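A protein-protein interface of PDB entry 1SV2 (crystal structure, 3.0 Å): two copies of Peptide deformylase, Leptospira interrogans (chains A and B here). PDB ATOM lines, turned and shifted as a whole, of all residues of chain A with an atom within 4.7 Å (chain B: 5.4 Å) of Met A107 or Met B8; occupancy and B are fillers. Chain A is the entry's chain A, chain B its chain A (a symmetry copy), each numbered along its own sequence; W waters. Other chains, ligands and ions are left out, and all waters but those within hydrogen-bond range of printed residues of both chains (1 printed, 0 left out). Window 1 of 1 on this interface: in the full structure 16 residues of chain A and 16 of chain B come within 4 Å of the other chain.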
ATOM      1  N   GLU A  99      12.348  26.554 -10.488  1.00  0.00           N
ATOM      2  CA  GLU A  99      13.401  27.438 -10.947  1.00  0.00           C
ATOM      3  C   GLU A  99      14.827  26.882 -10.817  1.00  0.00           C
ATOM      4  O   GLU A  99      15.113  25.991 -10.009  1.00  0.00           O
ATOM      5  CB  GLU A  99      13.299  28.789 -10.214  1.00  0.00           C
ATOM      6  CG  GLU A  99      12.296  29.755 -10.826  1.00  0.00           C
ATOM      7  CD  GLU A  99      12.198  31.080 -10.084  1.00  0.00           C
ATOM      8  OE1 GLU A  99      13.239  31.713  -9.791  1.00  0.00           O
ATOM      9  OE2 GLU A  99      11.062  31.498  -9.804  1.00  0.00           O
ATOM     10  N   GLY A 100      15.705  27.433 -11.648  1.00  0.00           N
ATOM     11  CA  GLY A 100      17.104  27.068 -11.644  1.00  0.00           C
ATOM     12  C   GLY A 100      17.866  28.351 -11.910  1.00  0.00           C
ATOM     13  O   GLY A 100      17.270  29.340 -12.336  1.00  0.00           O
ATOM     14  N   VAL A 104      23.722  28.909  -9.670  1.00  0.00           N
ATOM     15  CA  VAL A 104      23.438  27.827  -8.735  1.00  0.00           C
ATOM     16  C   VAL A 104      23.331  26.560  -9.572  1.00  0.00           C
ATOM     17  O   VAL A 104      22.258  25.968  -9.702  1.00  0.00           O
ATOM     18  CB  VAL A 104      22.114  28.074  -7.967  1.00  0.00           C
ATOM     19  CG1 VAL A 104      21.828  26.917  -7.029  1.00  0.00           C
ATOM     20  CG2 VAL A 104      22.219  29.346  -7.159  1.00  0.00           C
ATOM     21  N   PRO A 105      24.460  26.130 -10.149  1.00  0.00           N
ATOM     22  CA  PRO A 105      24.625  24.953 -11.003  1.00  0.00           C
ATOM     23  C   PRO A 105      24.047  23.615 -10.568  1.00  0.00           C
ATOM     24  O   PRO A 105      24.185  23.209  -9.422  1.00  0.00           O
ATOM     25  CB  PRO A 105      26.139  24.880 -11.192  1.00  0.00           C
ATOM     26  CG  PRO A 105      26.667  25.534  -9.979  1.00  0.00           C
ATOM     27  CD  PRO A 105      25.771  26.722  -9.854  1.00  0.00           C
ATOM     28  N   GLY A 106      23.398  22.947 -11.519  1.00  0.00           N
ATOM     29  CA  GLY A 106      22.823  21.629 -11.306  1.00  0.00           C
ATOM     30  C   GLY A 106      21.768  21.403 -10.242  1.00  0.00           C
ATOM     31  O   GLY A 106      21.644  20.286  -9.723  1.00  0.00           O
ATOM     32  N   MET A 107      20.994  22.429  -9.913  1.00  0.00           N
ATOM     33  CA  MET A 107      19.960  22.263  -8.901  1.00  0.00           C
ATOM     34  C   MET A 107      18.642  22.922  -9.280  1.00  0.00           C
ATOM     35  O   MET A 107      18.620  23.856 -10.076  1.00  0.00           O
ATOM     36  CB  MET A 107      20.455  22.816  -7.569  1.00  0.00           C
ATOM     37  CG  MET A 107      21.624  22.046  -7.009  1.00  0.00           C
ATOM     38  SD  MET A 107      22.291  22.873  -5.571  1.00  0.00           S
ATOM     39  CE  MET A 107      21.227  22.211  -4.292  1.00  0.00           C
ATOM     40  N   ARG A 108      17.548  22.426  -8.714  1.00  0.00           N
ATOM     41  CA  ARG A 108      16.227  22.979  -8.988  1.00  0.00           C
ATOM     42  C   ARG A 108      15.456  23.173  -7.702  1.00  0.00           C
ATOM     43  O   ARG A 108      15.589  22.392  -6.768  1.00  0.00           O
ATOM     44  CB  ARG A 108      15.422  22.059  -9.914  1.00  0.00           C
ATOM     45  CG  ARG A 108      15.955  21.973 -11.335  1.00  0.00           C
ATOM     46  CD  ARG A 108      16.058  23.352 -11.941  1.00  0.00           C
ATOM     47  NE  ARG A 108      17.028  23.398 -13.027  1.00  0.00           N
ATOM     48  CZ  ARG A 108      16.801  22.921 -14.244  1.00  0.00           C
ATOM     49  NH1 ARG A 108      15.623  22.361 -14.524  1.00  0.00           N
ATOM     50  NH2 ARG A 108      17.748  23.012 -15.176  1.00  0.00           N
ATOM     51  N   GLY A 109      14.641  24.217  -7.657  1.00  0.00           N
ATOM     52  CA  GLY A 109      13.857  24.473  -6.465  1.00  0.00           C
ATOM     53  C   GLY A 109      12.505  25.045  -6.817  1.00  0.00           C
ATOM     54  O   GLY A 109      12.411  25.993  -7.592  1.00  0.00           O
ATOM     55  N   TYR A 153      17.178  32.724  -6.040  1.00  0.00           N
ATOM     56  CA  TYR A 153      15.937  31.981  -5.852  1.00  0.00           C
ATOM     57  C   TYR A 153      15.913  31.058  -4.629  1.00  0.00           C
ATOM     58  O   TYR A 153      14.841  30.748  -4.102  1.00  0.00           O
ATOM     59  CB  TYR A 153      15.591  31.202  -7.124  1.00  0.00           C
ATOM     60  CG  TYR A 153      16.340  29.909  -7.305  1.00  0.00           C
ATOM     61  CD1 TYR A 153      15.788  28.698  -6.886  1.00  0.00           C
ATOM     62  CD2 TYR A 153      17.586  29.888  -7.921  1.00  0.00           C
ATOM     63  CE1 TYR A 153      16.456  27.488  -7.081  1.00  0.00           C
ATOM     64  CE2 TYR A 153      18.269  28.689  -8.122  1.00  0.00           C
ATOM     65  CZ  TYR A 153      17.696  27.488  -7.702  1.00  0.00           C
ATOM     66  OH  TYR A 153      18.362  26.298  -7.929  1.00  0.00           O
ATOM     67  N   PHE A 163      13.852  20.925  -3.090  1.00  0.00           N
ATOM     68  CA  PHE A 163      15.069  21.584  -3.522  1.00  0.00           C
ATOM     69  C   PHE A 163      16.109  20.473  -3.593  1.00  0.00           C
ATOM     70  O   PHE A 163      16.206  19.653  -2.679  1.00  0.00           O
ATOM     71  CB  PHE A 163      15.446  22.640  -2.478  1.00  0.00           C
ATOM     72  CG  PHE A 163      16.774  23.279  -2.700  1.00  0.00           C
ATOM     73  CD1 PHE A 163      17.188  23.639  -3.974  1.00  0.00           C
ATOM     74  CD2 PHE A 163      17.590  23.584  -1.619  1.00  0.00           C
ATOM     75  CE1 PHE A 163      18.399  24.300  -4.170  1.00  0.00           C
ATOM     76  CE2 PHE A 163      18.805  24.247  -1.797  1.00  0.00           C
ATOM     77  CZ  PHE A 163      19.210  24.607  -3.077  1.00  0.00           C
ATOM     78  N   GLY A 164      16.861  20.417  -4.685  1.00  0.00           N
ATOM     79  CA  GLY A 164      17.860  19.373  -4.814  1.00  0.00           C
ATOM     80  C   GLY A 164      18.623  19.427  -6.117  1.00  0.00           C
ATOM     81  O   GLY A 164      18.487  20.380  -6.880  1.00  0.00           O
ATOM     82  N   PHE A 165      19.433  18.403  -6.371  1.00  0.00           N
ATOM     83  CA  PHE A 165      20.222  18.344  -7.597  1.00  0.00           C
ATOM     84  C   PHE A 165      19.365  17.789  -8.726  1.00  0.00           C
ATOM     85  O   PHE A 165      18.506  16.934  -8.497  1.00  0.00           O
ATOM     86  CB  PHE A 165      21.462  17.478  -7.381  1.00  0.00           C
ATOM     87  CG  PHE A 165      22.350  17.970  -6.273  1.00  0.00           C
ATOM     88  CD1 PHE A 165      21.999  17.777  -4.942  1.00  0.00           C
ATOM     89  CD2 PHE A 165      23.514  18.666  -6.561  1.00  0.00           C
ATOM     90  CE1 PHE A 165      22.799  18.276  -3.916  1.00  0.00           C
ATOM     91  CE2 PHE A 165      24.320  19.170  -5.541  1.00  0.00           C
ATOM     92  CZ  PHE A 165      23.965  18.977  -4.217  1.00  0.00           C
ATOM     93  N   ASN A 166      19.593  18.291  -9.939  1.00  0.00           N
ATOM     94  CA  ASN A 166      18.825  17.872 -11.108  1.00  0.00           C
ATOM     95  C   ASN A 166      18.863  16.371 -11.257  1.00  0.00           C
ATOM     96  O   ASN A 166      17.824  15.700 -11.227  1.00  0.00           O
ATOM     97  CB  ASN A 166      19.397  18.512 -12.367  1.00  0.00           C
ATOM     98  CG  ASN A 166      19.427  20.018 -12.283  1.00  0.00           C
ATOM     99  OD1 ASN A 166      20.110  20.681 -13.062  1.00  0.00           O
ATOM    100  ND2 ASN A 166      18.681  20.572 -11.334  1.00  0.00           N
ATOM    101  N   THR A 168      19.318  13.743  -9.460  1.00  0.00           N
ATOM    102  CA  THR A 168      18.445  12.959  -8.596  1.00  0.00           C
ATOM    103  C   THR A 168      16.955  13.286  -8.644  1.00  0.00           C
ATOM    104  O   THR A 168      16.126  12.389  -8.527  1.00  0.00           O
ATOM    105  CB  THR A 168      18.899  13.052  -7.132  1.00  0.00           C
ATOM    106  OG1 THR A 168      18.256  14.165  -6.498  1.00  0.00           O
ATOM    107  CG2 THR A 168      20.410  13.237  -7.068  1.00  0.00           C
ATOM    108  N   LEU B   6      23.338   8.715  -1.459  1.00  0.00           N
ATOM    109  CA  LEU B   6      22.247   9.436  -2.100  1.00  0.00           C
ATOM    110  C   LEU B   6      22.412  10.957  -1.930  1.00  0.00           C
ATOM    111  O   LEU B   6      22.843  11.430  -0.870  1.00  0.00           O
ATOM    112  CB  LEU B   6      20.916   9.014  -1.490  1.00  0.00           C
ATOM    113  CG  LEU B   6      20.669   7.523  -1.288  1.00  0.00           C
ATOM    114  CD1 LEU B   6      19.272   7.342  -0.711  1.00  0.00           C
ATOM    115  CD2 LEU B   6      20.812   6.782  -2.602  1.00  0.00           C
ATOM    116  N   ARG B   7      22.058  11.719  -2.967  1.00  0.00           N
ATOM    117  CA  ARG B   7      22.179  13.174  -2.911  1.00  0.00           C
ATOM    118  C   ARG B   7      20.834  13.832  -2.644  1.00  0.00           C
ATOM    119  O   ARG B   7      19.778  13.221  -2.854  1.00  0.00           O
ATOM    120  CB  ARG B   7      22.772  13.714  -4.213  1.00  0.00           C
ATOM    121  CG  ARG B   7      24.117  13.090  -4.573  1.00  0.00           C
ATOM    122  CD  ARG B   7      24.904  13.927  -5.587  1.00  0.00           C
ATOM    123  NE  ARG B   7      24.147  14.154  -6.814  1.00  0.00           N
ATOM    124  CZ  ARG B   7      23.842  13.203  -7.695  1.00  0.00           C
ATOM    125  NH1 ARG B   7      24.240  11.950  -7.492  1.00  0.00           N
ATOM    126  NH2 ARG B   7      23.111  13.497  -8.769  1.00  0.00           N
ATOM    127  N   MET B   8      20.882  15.078  -2.174  1.00  0.00           N
ATOM    128  CA  MET B   8      19.669  15.837  -1.870  1.00  0.00           C
ATOM    129  C   MET B   8      18.762  15.908  -3.090  1.00  0.00           C
ATOM    130  O   MET B   8      19.206  16.219  -4.200  1.00  0.00           O
ATOM    131  CB  MET B   8      20.011  17.253  -1.399  1.00  0.00           C
ATOM    132  CG  MET B   8      18.780  18.081  -1.057  1.00  0.00           C
ATOM    133  SD  MET B   8      19.172  19.722  -0.426  1.00  0.00           S
ATOM    134  CE  MET B   8      20.132  20.345  -1.754  1.00  0.00           C
ATOM    135  N   GLY B   9      17.485  15.630  -2.874  1.00  0.00           N
ATOM    136  CA  GLY B   9      16.546  15.635  -3.968  1.00  0.00           C
ATOM    137  C   GLY B   9      15.954  14.247  -4.039  1.00  0.00           C
ATOM    138  O   GLY B   9      14.909  14.034  -4.646  1.00  0.00           O
ATOM    139  N   ASP B  10      16.635  13.288  -3.423  1.00  0.00           N
ATOM    140  CA  ASP B  10      16.142  11.917  -3.396  1.00  0.00           C
ATOM    141  C   ASP B  10      15.144  11.840  -2.248  1.00  0.00           C
ATOM    142  O   ASP B  10      15.460  12.155  -1.102  1.00  0.00           O
ATOM    143  CB  ASP B  10      17.283  10.939  -3.150  1.00  0.00           C
ATOM    144  CG  ASP B  10      16.854   9.497  -3.321  1.00  0.00           C
ATOM    145  OD1 ASP B  10      15.797   9.113  -2.755  1.00  0.00           O
ATOM    146  OD2 ASP B  10      17.583   8.755  -4.022  1.00  0.00           O
ATOM    147  N   LEU B  13      15.922  10.488   1.618  1.00  0.00           N
ATOM    148  CA  LEU B  13      16.491  11.401   2.593  1.00  0.00           C
ATOM    149  C   LEU B  13      15.461  12.207   3.353  1.00  0.00           C
ATOM    150  O   LEU B  13      15.818  12.944   4.259  1.00  0.00           O
ATOM    151  CB  LEU B  13      17.458  12.362   1.914  1.00  0.00           C
ATOM    152  CG  LEU B  13      18.665  11.729   1.221  1.00  0.00           C
ATOM    153  CD1 LEU B  13      19.457  12.799   0.491  1.00  0.00           C
ATOM    154  CD2 LEU B  13      19.547  11.035   2.239  1.00  0.00           C
ATOM    155  N   ARG B  14      14.190  12.083   3.004  1.00  0.00           N
ATOM    156  CA  ARG B  14      13.176  12.849   3.709  1.00  0.00           C
ATOM    157  C   ARG B  14      12.209  11.990   4.498  1.00  0.00           C
ATOM    158  O   ARG B  14      11.306  12.502   5.166  1.00  0.00           O
ATOM    159  CB  ARG B  14      12.392  13.707   2.728  1.00  0.00           C
ATOM    160  CG  ARG B  14      13.237  14.728   2.017  1.00  0.00           C
ATOM    161  CD  ARG B  14      13.693  15.797   2.961  1.00  0.00           C
ATOM    162  NE  ARG B  14      14.641  16.682   2.306  1.00  0.00           N
ATOM    163  CZ  ARG B  14      15.202  17.730   2.896  1.00  0.00           C
ATOM    164  NH1 ARG B  14      14.900  18.015   4.156  1.00  0.00           N
ATOM    165  NH2 ARG B  14      16.072  18.485   2.232  1.00  0.00           N
ATOM    166  N   SER B 103      25.666  14.229   1.307  1.00  0.00           N
ATOM    167  CA  SER B 103      24.487  14.128   0.450  1.00  0.00           C
ATOM    168  C   SER B 103      24.211  15.471  -0.214  1.00  0.00           C
ATOM    169  O   SER B 103      23.305  15.593  -1.041  1.00  0.00           O
ATOM    170  CB  SER B 103      23.260  13.696   1.261  1.00  0.00           C
ATOM    171  OG  SER B 103      23.395  12.373   1.749  1.00  0.00           O
ATOM    172  N   VAL B 104      24.993  16.477   0.169  1.00  0.00           N
ATOM    173  CA  VAL B 104      24.867  17.820  -0.381  1.00  0.00           C
ATOM    174  C   VAL B 104      26.274  18.259  -0.759  1.00  0.00           C
ATOM    175  O   VAL B 104      26.843  19.172  -0.159  1.00  0.00           O
ATOM    176  CB  VAL B 104      24.261  18.804   0.653  1.00  0.00           C
ATOM    177  CG1 VAL B 104      24.174  20.198   0.064  1.00  0.00           C
ATOM    178  CG2 VAL B 104      22.874  18.349   1.043  1.00  0.00           C
ATOM    179  N   MET B 107      29.150  22.047  -0.921  1.00  0.00           N
ATOM    180  CA  MET B 107      28.539  23.262  -0.398  1.00  0.00           C
ATOM    181  C   MET B 107      28.642  23.376   1.116  1.00  0.00           C
ATOM    182  O   MET B 107      28.775  22.371   1.809  1.00  0.00           O
ATOM    183  CB  MET B 107      27.078  23.324  -0.826  1.00  0.00           C
ATOM    184  CG  MET B 107      26.906  23.459  -2.318  1.00  0.00           C
ATOM    185  SD  MET B 107      25.183  23.305  -2.770  1.00  0.00           S
ATOM    186  CE  MET B 107      24.635  24.994  -2.542  1.00  0.00           C
ATOM    187  N   LEU B 152      17.686  17.595   6.479  1.00  0.00           N
ATOM    188  CA  LEU B 152      19.023  17.924   5.995  1.00  0.00           C
ATOM    189  C   LEU B 152      19.391  19.281   6.573  1.00  0.00           C
ATOM    190  O   LEU B 152      18.507  20.060   6.916  1.00  0.00           O
ATOM    191  CB  LEU B 152      19.039  17.975   4.471  1.00  0.00           C
ATOM    192  CG  LEU B 152      18.559  16.700   3.771  1.00  0.00           C
ATOM    193  CD1 LEU B 152      18.907  16.816   2.286  1.00  0.00           C
ATOM    194  CD2 LEU B 152      19.219  15.453   4.385  1.00  0.00           C
ATOM    195  N   VAL B 154      20.328  21.961   5.223  1.00  0.00           N
ATOM    196  CA  VAL B 154      19.844  23.109   4.461  1.00  0.00           C
ATOM    197  C   VAL B 154      18.499  23.539   5.022  1.00  0.00           C
ATOM    198  O   VAL B 154      18.034  24.639   4.747  1.00  0.00           O
ATOM    199  CB  VAL B 154      19.671  22.796   2.952  1.00  0.00           C
ATOM    200  CG1 VAL B 154      20.987  22.330   2.357  1.00  0.00           C
ATOM    201  CG2 VAL B 154      18.611  21.749   2.755  1.00  0.00           C
ATOM    202  N   PHE B 165      28.688  27.363  -2.574  1.00  0.00           N
ATOM    203  CA  PHE B 165      29.630  26.319  -2.965  1.00  0.00           C
ATOM    204  C   PHE B 165      30.970  26.565  -2.287  1.00  0.00           C
ATOM    205  O   PHE B 165      31.366  27.716  -2.083  1.00  0.00           O
ATOM    206  CB  PHE B 165      29.786  26.296  -4.484  1.00  0.00           C
ATOM    207  CG  PHE B 165      28.493  26.061  -5.215  1.00  0.00           C
ATOM    208  CD1 PHE B 165      27.552  27.076  -5.339  1.00  0.00           C
ATOM    209  CD2 PHE B 165      28.197  24.811  -5.738  1.00  0.00           C
ATOM    210  CE1 PHE B 165      26.334  26.844  -5.974  1.00  0.00           C
ATOM    211  CE2 PHE B 165      26.981  24.569  -6.374  1.00  0.00           C
ATOM    212  CZ  PHE B 165      26.047  25.583  -6.494  1.00  0.00           C
HETATM  213  O   HOH W   1      15.471  18.436  -0.618  1.00  0.00           O
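N of Phe A165 sits at hydrogen-bond distance from O of Met B8 (3.1 Å).
OG1 of Thr A168 sits at hydrogen-bond distance from O of Met B8 (3.2 Å).
O of Phe A163 sits close to SD of Met B8 (3.7 Å).
The backbone carbonyl oxygen of Met A107 sits at hydrogen-bond distance from the side-chain hydroxyl of Tyr A153, at 3.3 Å.
N of Met A107 lies close to ND2 of Asn A166.
O of Gly A164 lies within hydrogen-bond range of N of Arg A108.
O of Phe A165 sits at hydrogen-bond distance from OG1 of Thr A168, at 3.4 Å.
O of Leu B6 sits at hydrogen-bond distance from OG of Ser B103 (2.8 Å).
O of Ser B103 lies within hydrogen-bond range of N of Met B8.
Among the printed residues, pairs that only touch across the chains: Pro A105 with Phe B165 (3.5 Å), Met A107 with Met B8 (3.3 Å), Gly A164 with Met B8 (3.5 Å), Phe A165 with Ser B103 (3.96 Å), Thr A168 with Arg B7 (3.2 Å), Thr A168 with Gly B9 (3.4 Å) and Thr A168 with Asp B10 (3.6 Å).
Of the printed residues of chain B, Met A107 touches Met B8.
Printed residues of chain B within 4 Å of Gly A164: Met B8.
Of the printed residues of chain A, Arg B7 touches Thr A168.
Printed residues of chain B within 4 Å of Pro A105: Phe B165.
Val B104 touches none of the printed residues of chain A.
The nearest residue of chain B that does not touch Met A107 is Met B107 (4.05 Å).
The nearest printed residue of chain B that does not touch Gly A164 is Gly B9 (4.1 Å).
Along chain A the printed residues that touch a printed residue of chain B span positions 105 to 168.
Among the printed residues, 10 pairs touch across the chains.
Positions printed for both chains: 104, 107 and 165.
Of the 10 pairs that touch across the chains among the printed residues, none has its exchanged pair printed and touching as well.
Water W1 lies within hydrogen-bond range of the backbone carbonyl oxygen of Phe A163 (2.5 Å) and the guanidinium group of Arg B14 (2.9 Å).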
